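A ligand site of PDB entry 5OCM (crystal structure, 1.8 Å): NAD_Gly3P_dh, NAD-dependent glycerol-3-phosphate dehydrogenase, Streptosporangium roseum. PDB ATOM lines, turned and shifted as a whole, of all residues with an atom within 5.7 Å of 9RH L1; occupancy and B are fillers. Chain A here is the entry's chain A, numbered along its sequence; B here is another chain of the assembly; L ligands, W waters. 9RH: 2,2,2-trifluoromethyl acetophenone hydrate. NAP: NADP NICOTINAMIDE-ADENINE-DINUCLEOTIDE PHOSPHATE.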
ATOM      1  N   TRP A 208     -27.180   4.266  33.542  1.00  0.00           N
ATOM      2  CA  TRP A 208     -26.839   5.375  32.686  1.00  0.00           C
ATOM      3  C   TRP A 208     -27.946   6.458  32.638  1.00  0.00           C
ATOM      4  O   TRP A 208     -27.667   7.665  32.725  1.00  0.00           O
ATOM      5  CB  TRP A 208     -26.513   4.865  31.273  1.00  0.00           C
ATOM      6  CG  TRP A 208     -26.205   5.914  30.291  1.00  0.00           C
ATOM      7  CD1 TRP A 208     -26.786   6.065  29.105  1.00  0.00           C
ATOM      8  CD2 TRP A 208     -25.172   6.927  30.374  1.00  0.00           C
ATOM      9  NE1 TRP A 208     -26.232   7.121  28.433  1.00  0.00           N
ATOM     10  CE2 TRP A 208     -25.207   7.642  29.179  1.00  0.00           C
ATOM     11  CE3 TRP A 208     -24.214   7.275  31.338  1.00  0.00           C
ATOM     12  CZ2 TRP A 208     -24.368   8.730  28.920  1.00  0.00           C
ATOM     13  CZ3 TRP A 208     -23.349   8.368  31.065  1.00  0.00           C
ATOM     14  CH2 TRP A 208     -23.459   9.090  29.853  1.00  0.00           C
ATOM     15  N   PHE A 215     -27.347  15.506  33.863  1.00  0.00           N
ATOM     16  CA  PHE A 215     -27.180  16.353  32.697  1.00  0.00           C
ATOM     17  C   PHE A 215     -28.440  17.176  32.478  1.00  0.00           C
ATOM     18  O   PHE A 215     -28.369  18.359  32.171  1.00  0.00           O
ATOM     19  CB  PHE A 215     -26.874  15.582  31.393  1.00  0.00           C
ATOM     20  CG  PHE A 215     -25.842  14.467  31.513  1.00  0.00           C
ATOM     21  CD1 PHE A 215     -24.901  14.463  32.499  1.00  0.00           C
ATOM     22  CD2 PHE A 215     -25.839  13.471  30.573  1.00  0.00           C
ATOM     23  CE1 PHE A 215     -23.990  13.410  32.615  1.00  0.00           C
ATOM     24  CE2 PHE A 215     -24.921  12.420  30.659  1.00  0.00           C
ATOM     25  CZ  PHE A 215     -24.030  12.388  31.713  1.00  0.00           C
ATOM     26  N   TYR A 219     -28.234  21.206  32.272  1.00  0.00           N
ATOM     27  CA  TYR A 219     -28.613  21.796  31.003  1.00  0.00           C
ATOM     28  C   TYR A 219     -29.835  22.674  31.201  1.00  0.00           C
ATOM     29  O   TYR A 219     -29.977  23.708  30.520  1.00  0.00           O
ATOM     30  CB  TYR A 219     -28.788  20.758  29.912  1.00  0.00           C
ATOM     31  CG  TYR A 219     -27.507  19.993  29.583  1.00  0.00           C
ATOM     32  CD1 TYR A 219     -26.260  20.335  30.154  1.00  0.00           C
ATOM     33  CD2 TYR A 219     -27.549  18.957  28.679  1.00  0.00           C
ATOM     34  CE1 TYR A 219     -25.113  19.542  29.872  1.00  0.00           C
ATOM     35  CE2 TYR A 219     -26.409  18.186  28.408  1.00  0.00           C
ATOM     36  CZ  TYR A 219     -25.223  18.485  28.991  1.00  0.00           C
ATOM     37  OH  TYR A 219     -24.132  17.678  28.715  1.00  0.00           O
ATOM     38  N   ASP A 232     -18.731  20.051  29.864  1.00  0.00           N
ATOM     39  CA  ASP A 232     -18.517  18.602  29.788  1.00  0.00           C
ATOM     40  C   ASP A 232     -18.031  18.160  28.440  1.00  0.00           C
ATOM     41  O   ASP A 232     -16.939  17.579  28.336  1.00  0.00           O
ATOM     42  CB  ASP A 232     -19.760  17.767  30.266  1.00  0.00           C
ATOM     43  CG  ASP A 232     -21.117  18.345  29.737  1.00  0.00           C
ATOM     44  OD1 ASP A 232     -21.139  19.168  28.791  1.00  0.00           O
ATOM     45  OD2 ASP A 232     -22.146  17.901  30.296  1.00  0.00           O
ATOM     46  N   ALA A 233     -18.814  18.428  27.389  1.00  0.00           N
ATOM     47  CA  ALA A 233     -18.540  17.997  26.041  1.00  0.00           C
ATOM     48  C   ALA A 233     -19.142  18.998  25.068  1.00  0.00           C
ATOM     49  O   ALA A 233     -20.262  19.498  25.293  1.00  0.00           O
ATOM     50  CB  ALA A 233     -19.155  16.623  25.786  1.00  0.00           C
ATOM     51  N   THR A 234     -18.466  19.278  23.965  1.00  0.00           N
ATOM     52  CA  THR A 234     -19.007  20.106  22.912  1.00  0.00           C
ATOM     53  C   THR A 234     -19.978  19.326  22.015  1.00  0.00           C
ATOM     54  O   THR A 234     -19.946  18.065  21.919  1.00  0.00           O
ATOM     55  CB  THR A 234     -17.879  20.633  21.991  1.00  0.00           C
ATOM     56  OG1 THR A 234     -17.209  19.525  21.392  1.00  0.00           O
ATOM     57  CG2 THR A 234     -16.843  21.445  22.761  1.00  0.00           C
ATOM     58  N   THR A 237     -18.096  17.113  19.733  1.00  0.00           N
ATOM     59  CA  THR A 237     -17.708  15.840  20.343  1.00  0.00           C
ATOM     60  C   THR A 237     -18.914  14.864  20.365  1.00  0.00           C
ATOM     61  O   THR A 237     -18.777  13.665  20.021  1.00  0.00           O
ATOM     62  CB  THR A 237     -17.154  16.085  21.758  1.00  0.00           C
ATOM     63  OG1 THR A 237     -15.969  16.852  21.633  1.00  0.00           O
ATOM     64  CG2 THR A 237     -16.846  14.854  22.486  1.00  0.00           C
ATOM     65  N   HIS A 238     -20.082  15.382  20.746  1.00  0.00           N
ATOM     66  CA  HIS A 238     -21.310  14.598  20.632  1.00  0.00           C
ATOM     67  C   HIS A 238     -21.511  13.988  19.225  1.00  0.00           C
ATOM     68  O   HIS A 238     -21.805  12.789  19.084  1.00  0.00           O
ATOM     69  CB  HIS A 238     -22.576  15.426  21.011  1.00  0.00           C
ATOM     70  CG  HIS A 238     -22.798  15.589  22.497  1.00  0.00           C
ATOM     71  ND1 HIS A 238     -23.571  14.703  23.231  1.00  0.00           N
ATOM     72  CD2 HIS A 238     -22.420  16.563  23.365  1.00  0.00           C
ATOM     73  CE1 HIS A 238     -23.650  15.151  24.484  1.00  0.00           C
ATOM     74  NE2 HIS A 238     -22.972  16.272  24.591  1.00  0.00           N
ATOM     75  N   THR A 241     -19.678  10.911  18.220  1.00  0.00           N
ATOM     76  CA  THR A 241     -20.269   9.658  18.775  1.00  0.00           C
ATOM     77  C   THR A 241     -21.603   9.313  18.162  1.00  0.00           C
ATOM     78  O   THR A 241     -21.926   8.135  18.067  1.00  0.00           O
ATOM     79  CB  THR A 241     -20.330   9.658  20.330  1.00  0.00           C
ATOM     80  OG1 THR A 241     -20.857  10.916  20.810  1.00  0.00           O
ATOM     81  CG2 THR A 241     -18.964   9.470  20.901  1.00  0.00           C
ATOM     82  N   SER B  94     -13.614   7.216  22.426  1.00  0.00           N
ATOM     83  CA  SER B  94     -14.834   6.695  21.818  1.00  0.00           C
ATOM     84  C   SER B  94     -14.540   6.125  20.402  1.00  0.00           C
ATOM     85  O   SER B  94     -13.622   6.575  19.691  1.00  0.00           O
ATOM     86  CB  SER B  94     -15.907   7.800  21.645  1.00  0.00           C
ATOM     87  OG  SER B  94     -16.042   8.521  22.843  1.00  0.00           O
ATOM     88  N   ILE B 119     -16.077   5.389  28.849  1.00  0.00           N
ATOM     89  CA  ILE B 119     -16.307   6.191  30.040  1.00  0.00           C
ATOM     90  C   ILE B 119     -17.770   6.654  29.971  1.00  0.00           C
ATOM     91  O   ILE B 119     -18.140   7.475  29.125  1.00  0.00           O
ATOM     92  CB  ILE B 119     -15.437   7.474  30.051  1.00  0.00           C
ATOM     93  CG1 ILE B 119     -13.963   7.113  29.964  1.00  0.00           C
ATOM     94  CG2 ILE B 119     -15.673   8.303  31.324  1.00  0.00           C
ATOM     95  CD1 ILE B 119     -13.118   8.265  29.443  1.00  0.00           C
ATOM     96  N   MET B 120     -18.580   6.102  30.866  1.00  0.00           N
ATOM     97  CA  MET B 120     -20.003   6.432  30.901  1.00  0.00           C
ATOM     98  C   MET B 120     -20.177   7.462  32.029  1.00  0.00           C
ATOM     99  O   MET B 120     -20.792   7.221  33.088  1.00  0.00           O
ATOM    100  CB  MET B 120     -20.889   5.187  31.147  1.00  0.00           C
ATOM    101  CG  MET B 120     -20.618   4.032  30.167  1.00  0.00           C
ATOM    102  SD  MET B 120     -20.452   4.431  28.441  1.00  0.00           S
ATOM    103  CE  MET B 120     -21.980   5.341  28.142  1.00  0.00           C
ATOM    104  N   ALA B 121     -19.630   8.625  31.755  1.00  0.00           N
ATOM    105  CA  ALA B 121     -19.591   9.750  32.706  1.00  0.00           C
ATOM    106  C   ALA B 121     -19.135  11.001  31.972  1.00  0.00           C
ATOM    107  O   ALA B 121     -18.385  10.913  30.963  1.00  0.00           O
ATOM    108  CB  ALA B 121     -18.629   9.469  33.831  1.00  0.00           C
ATOM    109  N   ILE B 122     -19.514  12.136  32.510  1.00  0.00           N
ATOM    110  CA  ILE B 122     -18.918  13.410  32.143  1.00  0.00           C
ATOM    111  C   ILE B 122     -17.649  13.699  33.025  1.00  0.00           C
ATOM    112  O   ILE B 122     -17.437  13.071  34.094  1.00  0.00           O
ATOM    113  CB  ILE B 122     -19.892  14.580  32.289  1.00  0.00           C
ATOM    114  CG1 ILE B 122     -20.496  14.674  33.686  1.00  0.00           C
ATOM    115  CG2 ILE B 122     -20.965  14.480  31.190  1.00  0.00           C
ATOM    116  CD1 ILE B 122     -21.321  15.946  33.938  1.00  0.00           C
ATOM    117  N   LEU B 174     -25.186   5.707  24.661  1.00  0.00           N
ATOM    118  CA  LEU B 174     -25.207   7.096  24.243  1.00  0.00           C
ATOM    119  C   LEU B 174     -26.470   7.448  23.483  1.00  0.00           C
ATOM    120  O   LEU B 174     -27.008   8.579  23.630  1.00  0.00           O
ATOM    121  CB  LEU B 174     -23.937   7.439  23.426  1.00  0.00           C
ATOM    122  CG  LEU B 174     -22.622   7.318  24.175  1.00  0.00           C
ATOM    123  CD1 LEU B 174     -21.480   7.694  23.236  1.00  0.00           C
ATOM    124  CD2 LEU B 174     -22.611   8.160  25.439  1.00  0.00           C
ATOM    125  N   MET B 177     -28.910   8.540  25.936  1.00  0.00           N
ATOM    126  CA  MET B 177     -28.671   9.934  26.336  1.00  0.00           C
ATOM    127  C   MET B 177     -29.300  10.931  25.377  1.00  0.00           C
ATOM    128  O   MET B 177     -29.981  11.880  25.806  1.00  0.00           O
ATOM    129  CB  MET B 177     -27.157  10.192  26.522  1.00  0.00           C
ATOM    130  CG  MET B 177     -26.822  11.648  26.745  1.00  0.00           C
ATOM    131  SD  MET B 177     -25.070  11.972  26.912  1.00  0.00           S
ATOM    132  CE  MET B 177     -24.537  11.663  25.214  1.00  0.00           C
ATOM    133  N   TRP B 178     -29.078  10.749  24.066  1.00  0.00           N
ATOM    134  CA  TRP B 178     -29.664  11.739  23.106  1.00  0.00           C
ATOM    135  C   TRP B 178     -31.173  11.662  23.100  1.00  0.00           C
ATOM    136  O   TRP B 178     -31.842  12.703  23.012  1.00  0.00           O
ATOM    137  CB  TRP B 178     -29.063  11.640  21.688  1.00  0.00           C
ATOM    138  CG  TRP B 178     -27.565  11.869  21.703  1.00  0.00           C
ATOM    139  CD1 TRP B 178     -26.907  12.942  22.204  1.00  0.00           C
ATOM    140  CD2 TRP B 178     -26.569  10.977  21.232  1.00  0.00           C
ATOM    141  NE1 TRP B 178     -25.581  12.780  22.085  1.00  0.00           N
ATOM    142  CE2 TRP B 178     -25.329  11.567  21.520  1.00  0.00           C
ATOM    143  CE3 TRP B 178     -26.610   9.713  20.622  1.00  0.00           C
ATOM    144  CZ2 TRP B 178     -24.125  10.934  21.213  1.00  0.00           C
ATOM    145  CZ3 TRP B 178     -25.428   9.103  20.331  1.00  0.00           C
ATOM    146  CH2 TRP B 178     -24.202   9.709  20.628  1.00  0.00           C
HETATM  147  O1  9RH L   1     -20.661  13.508  23.737  1.00  0.00           O
HETATM  148  C1  9RH L   1     -20.431  12.177  24.252  1.00  0.00           C
HETATM  149  O2  9RH L   1     -21.196  11.186  23.607  1.00  0.00           O
HETATM  150  C2  9RH L   1     -20.693  12.091  25.751  1.00  0.00           C
HETATM  151  C3  9RH L   1     -21.064  13.222  26.445  1.00  0.00           C
HETATM  152  C4  9RH L   1     -21.430  13.135  27.784  1.00  0.00           C
HETATM  153  C5  9RH L   1     -21.386  11.932  28.439  1.00  0.00           C
HETATM  154  C6  9RH L   1     -20.990  10.795  27.760  1.00  0.00           C
HETATM  155  C7  9RH L   1     -20.654  10.874  26.413  1.00  0.00           C
HETATM  156  C8  9RH L   1     -18.969  11.924  23.985  1.00  0.00           C
HETATM  157  F1  9RH L   1     -18.706  12.102  22.679  1.00  0.00           F
HETATM  158  F2  9RH L   1     -18.591  10.671  24.367  1.00  0.00           F
HETATM  159  F3  9RH L   1     -18.299  12.806  24.701  1.00  0.00           F
HETATM  160  PA  NAP L   2     -11.534  17.150  23.608  1.00  0.00           P
HETATM  161  O1A NAP L   2     -11.919  17.523  22.167  1.00  0.00           O
HETATM  162  O2A NAP L   2     -11.699  18.159  24.716  1.00  0.00           O
HETATM  163  O5B NAP L   2     -10.035  16.446  23.595  1.00  0.00           O
HETATM  164  C5B NAP L   2      -9.638  15.753  22.433  1.00  0.00           C
HETATM  165  C4B NAP L   2      -8.203  15.294  22.753  1.00  0.00           C
HETATM  166  O4B NAP L   2      -7.755  14.541  21.610  1.00  0.00           O
HETATM  167  C3B NAP L   2      -7.138  16.380  22.973  1.00  0.00           C
HETATM  168  O3B NAP L   2      -6.234  15.858  23.942  1.00  0.00           O
HETATM  169  C2B NAP L   2      -6.487  16.515  21.585  1.00  0.00           C
HETATM  170  O2B NAP L   2      -5.201  17.046  21.570  1.00  0.00           O
HETATM  171  C1B NAP L   2      -6.443  15.052  21.218  1.00  0.00           C
HETATM  172  N9A NAP L   2      -6.233  14.827  19.797  1.00  0.00           N
HETATM  173  C8A NAP L   2      -7.075  15.120  18.795  1.00  0.00           C
HETATM  174  N7A NAP L   2      -6.490  14.801  17.625  1.00  0.00           N
HETATM  175  C5A NAP L   2      -5.235  14.334  17.889  1.00  0.00           C
HETATM  176  C6A NAP L   2      -4.102  13.861  17.091  1.00  0.00           C
HETATM  177  N6A NAP L   2      -4.266  13.825  15.777  1.00  0.00           N
HETATM  178  N1A NAP L   2      -2.964  13.530  17.709  1.00  0.00           N
HETATM  179  C2A NAP L   2      -2.869  13.581  19.047  1.00  0.00           C
HETATM  180  N3A NAP L   2      -3.882  14.042  19.854  1.00  0.00           N
HETATM  181  C4A NAP L   2      -5.041  14.425  19.307  1.00  0.00           C
HETATM  182  O3  NAP L   2     -12.346  15.829  23.794  1.00  0.00           O
HETATM  183  PN  NAP L   2     -12.732  15.133  25.196  1.00  0.00           P
HETATM  184  O1N NAP L   2     -14.042  15.641  25.737  1.00  0.00           O
HETATM  185  O2N NAP L   2     -11.533  15.069  26.107  1.00  0.00           O
HETATM  186  O5D NAP L   2     -13.036  13.712  24.612  1.00  0.00           O
HETATM  187  C5D NAP L   2     -12.021  12.674  24.517  1.00  0.00           C
HETATM  188  C4D NAP L   2     -12.587  11.352  24.186  1.00  0.00           C
HETATM  189  O4D NAP L   2     -13.330  10.897  25.342  1.00  0.00           O
HETATM  190  C3D NAP L   2     -13.569  11.382  23.016  1.00  0.00           C
HETATM  191  O3D NAP L   2     -13.431  10.141  22.349  1.00  0.00           O
HETATM  192  C2D NAP L   2     -14.960  11.452  23.659  1.00  0.00           C
HETATM  193  O2D NAP L   2     -16.025  11.011  22.764  1.00  0.00           O
HETATM  194  C1D NAP L   2     -14.712  10.673  24.932  1.00  0.00           C
HETATM  195  N1N NAP L   2     -15.653  11.018  26.037  1.00  0.00           N
HETATM  196  C2N NAP L   2     -15.844  12.289  26.384  1.00  0.00           C
HETATM  197  C3N NAP L   2     -16.722  12.679  27.384  1.00  0.00           C
HETATM  198  C7N NAP L   2     -16.982  14.105  27.798  1.00  0.00           C
HETATM  199  O7N NAP L   2     -18.036  14.315  28.462  1.00  0.00           O
HETATM  200  N7N NAP L   2     -16.103  15.053  27.446  1.00  0.00           N
HETATM  201  C4N NAP L   2     -17.478  11.670  27.980  1.00  0.00           C
HETATM  202  C5N NAP L   2     -17.278  10.305  27.618  1.00  0.00           C
HETATM  203  C6N NAP L   2     -16.376   9.979  26.597  1.00  0.00           C
HETATM  204  P2B NAP L   2      -4.971  18.638  21.435  1.00  0.00           P
HETATM  205  O1X NAP L   2      -5.242  19.242  22.777  1.00  0.00           O
HETATM  206  O2X NAP L   2      -3.590  18.698  20.934  1.00  0.00           O
HETATM  207  O3X NAP L   2      -5.993  19.100  20.453  1.00  0.00           O
HETATM  208  O   HOH W   1     -16.355  12.044  20.302  1.00  0.00           O
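An oxygen (O2) of 9RH L1 is in hydrogen-bond range of the side-chain hydroxyl of Thr 241 (2.8 Å).
A ring nitrogen (ND1) of His 238 is in hydrogen-bond range of an oxygen (O1) of 9RH L1 (3.2 Å).
The backbone NH (N) of Ser 94 of chain B sits at hydrogen-bond distance from an oxygen (O3D) of NAP L2, 2.9 Å away.
An oxygen (O2D) of NAP L2 sits at hydrogen-bond distance from the side-chain hydroxyl (OG) of Ser 94 of chain B (2.5 Å).
The backbone carbonyl oxygen (O) of Asp 232 is in hydrogen-bond range of a nitrogen (N7N) of NAP L2 (2.8 Å).
The side-chain hydroxyl (OG1) of Thr 241 is in hydrogen-bond range of the backbone carbonyl oxygen (O) of His 238 (2.7 Å).
The side-chain hydroxyl (OG1) of Thr 234 sits at hydrogen-bond distance from the side-chain hydroxyl (OG1) of Thr 237 (3.0 Å).
A ring nitrogen (ND1) of His 238 sits at hydrogen-bond distance from the indole nitrogen (NE1) of Trp 178 of chain B.
A fluorine (F1) of 9RH L1 sits close to the backbone carbonyl oxygen of Thr 237 (3.1 Å).
Merely in contact with 9RH L1: Leu 174 of chain B, Trp 208, Ser 94 of chain B, Ile 122 of chain B, Met 177 of chain B, Trp 178 of chain B and Ala 233.
Water W1 bridges an oxygen (O2D) of NAP L2 and the backbone carbonyl oxygen of Thr 237.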
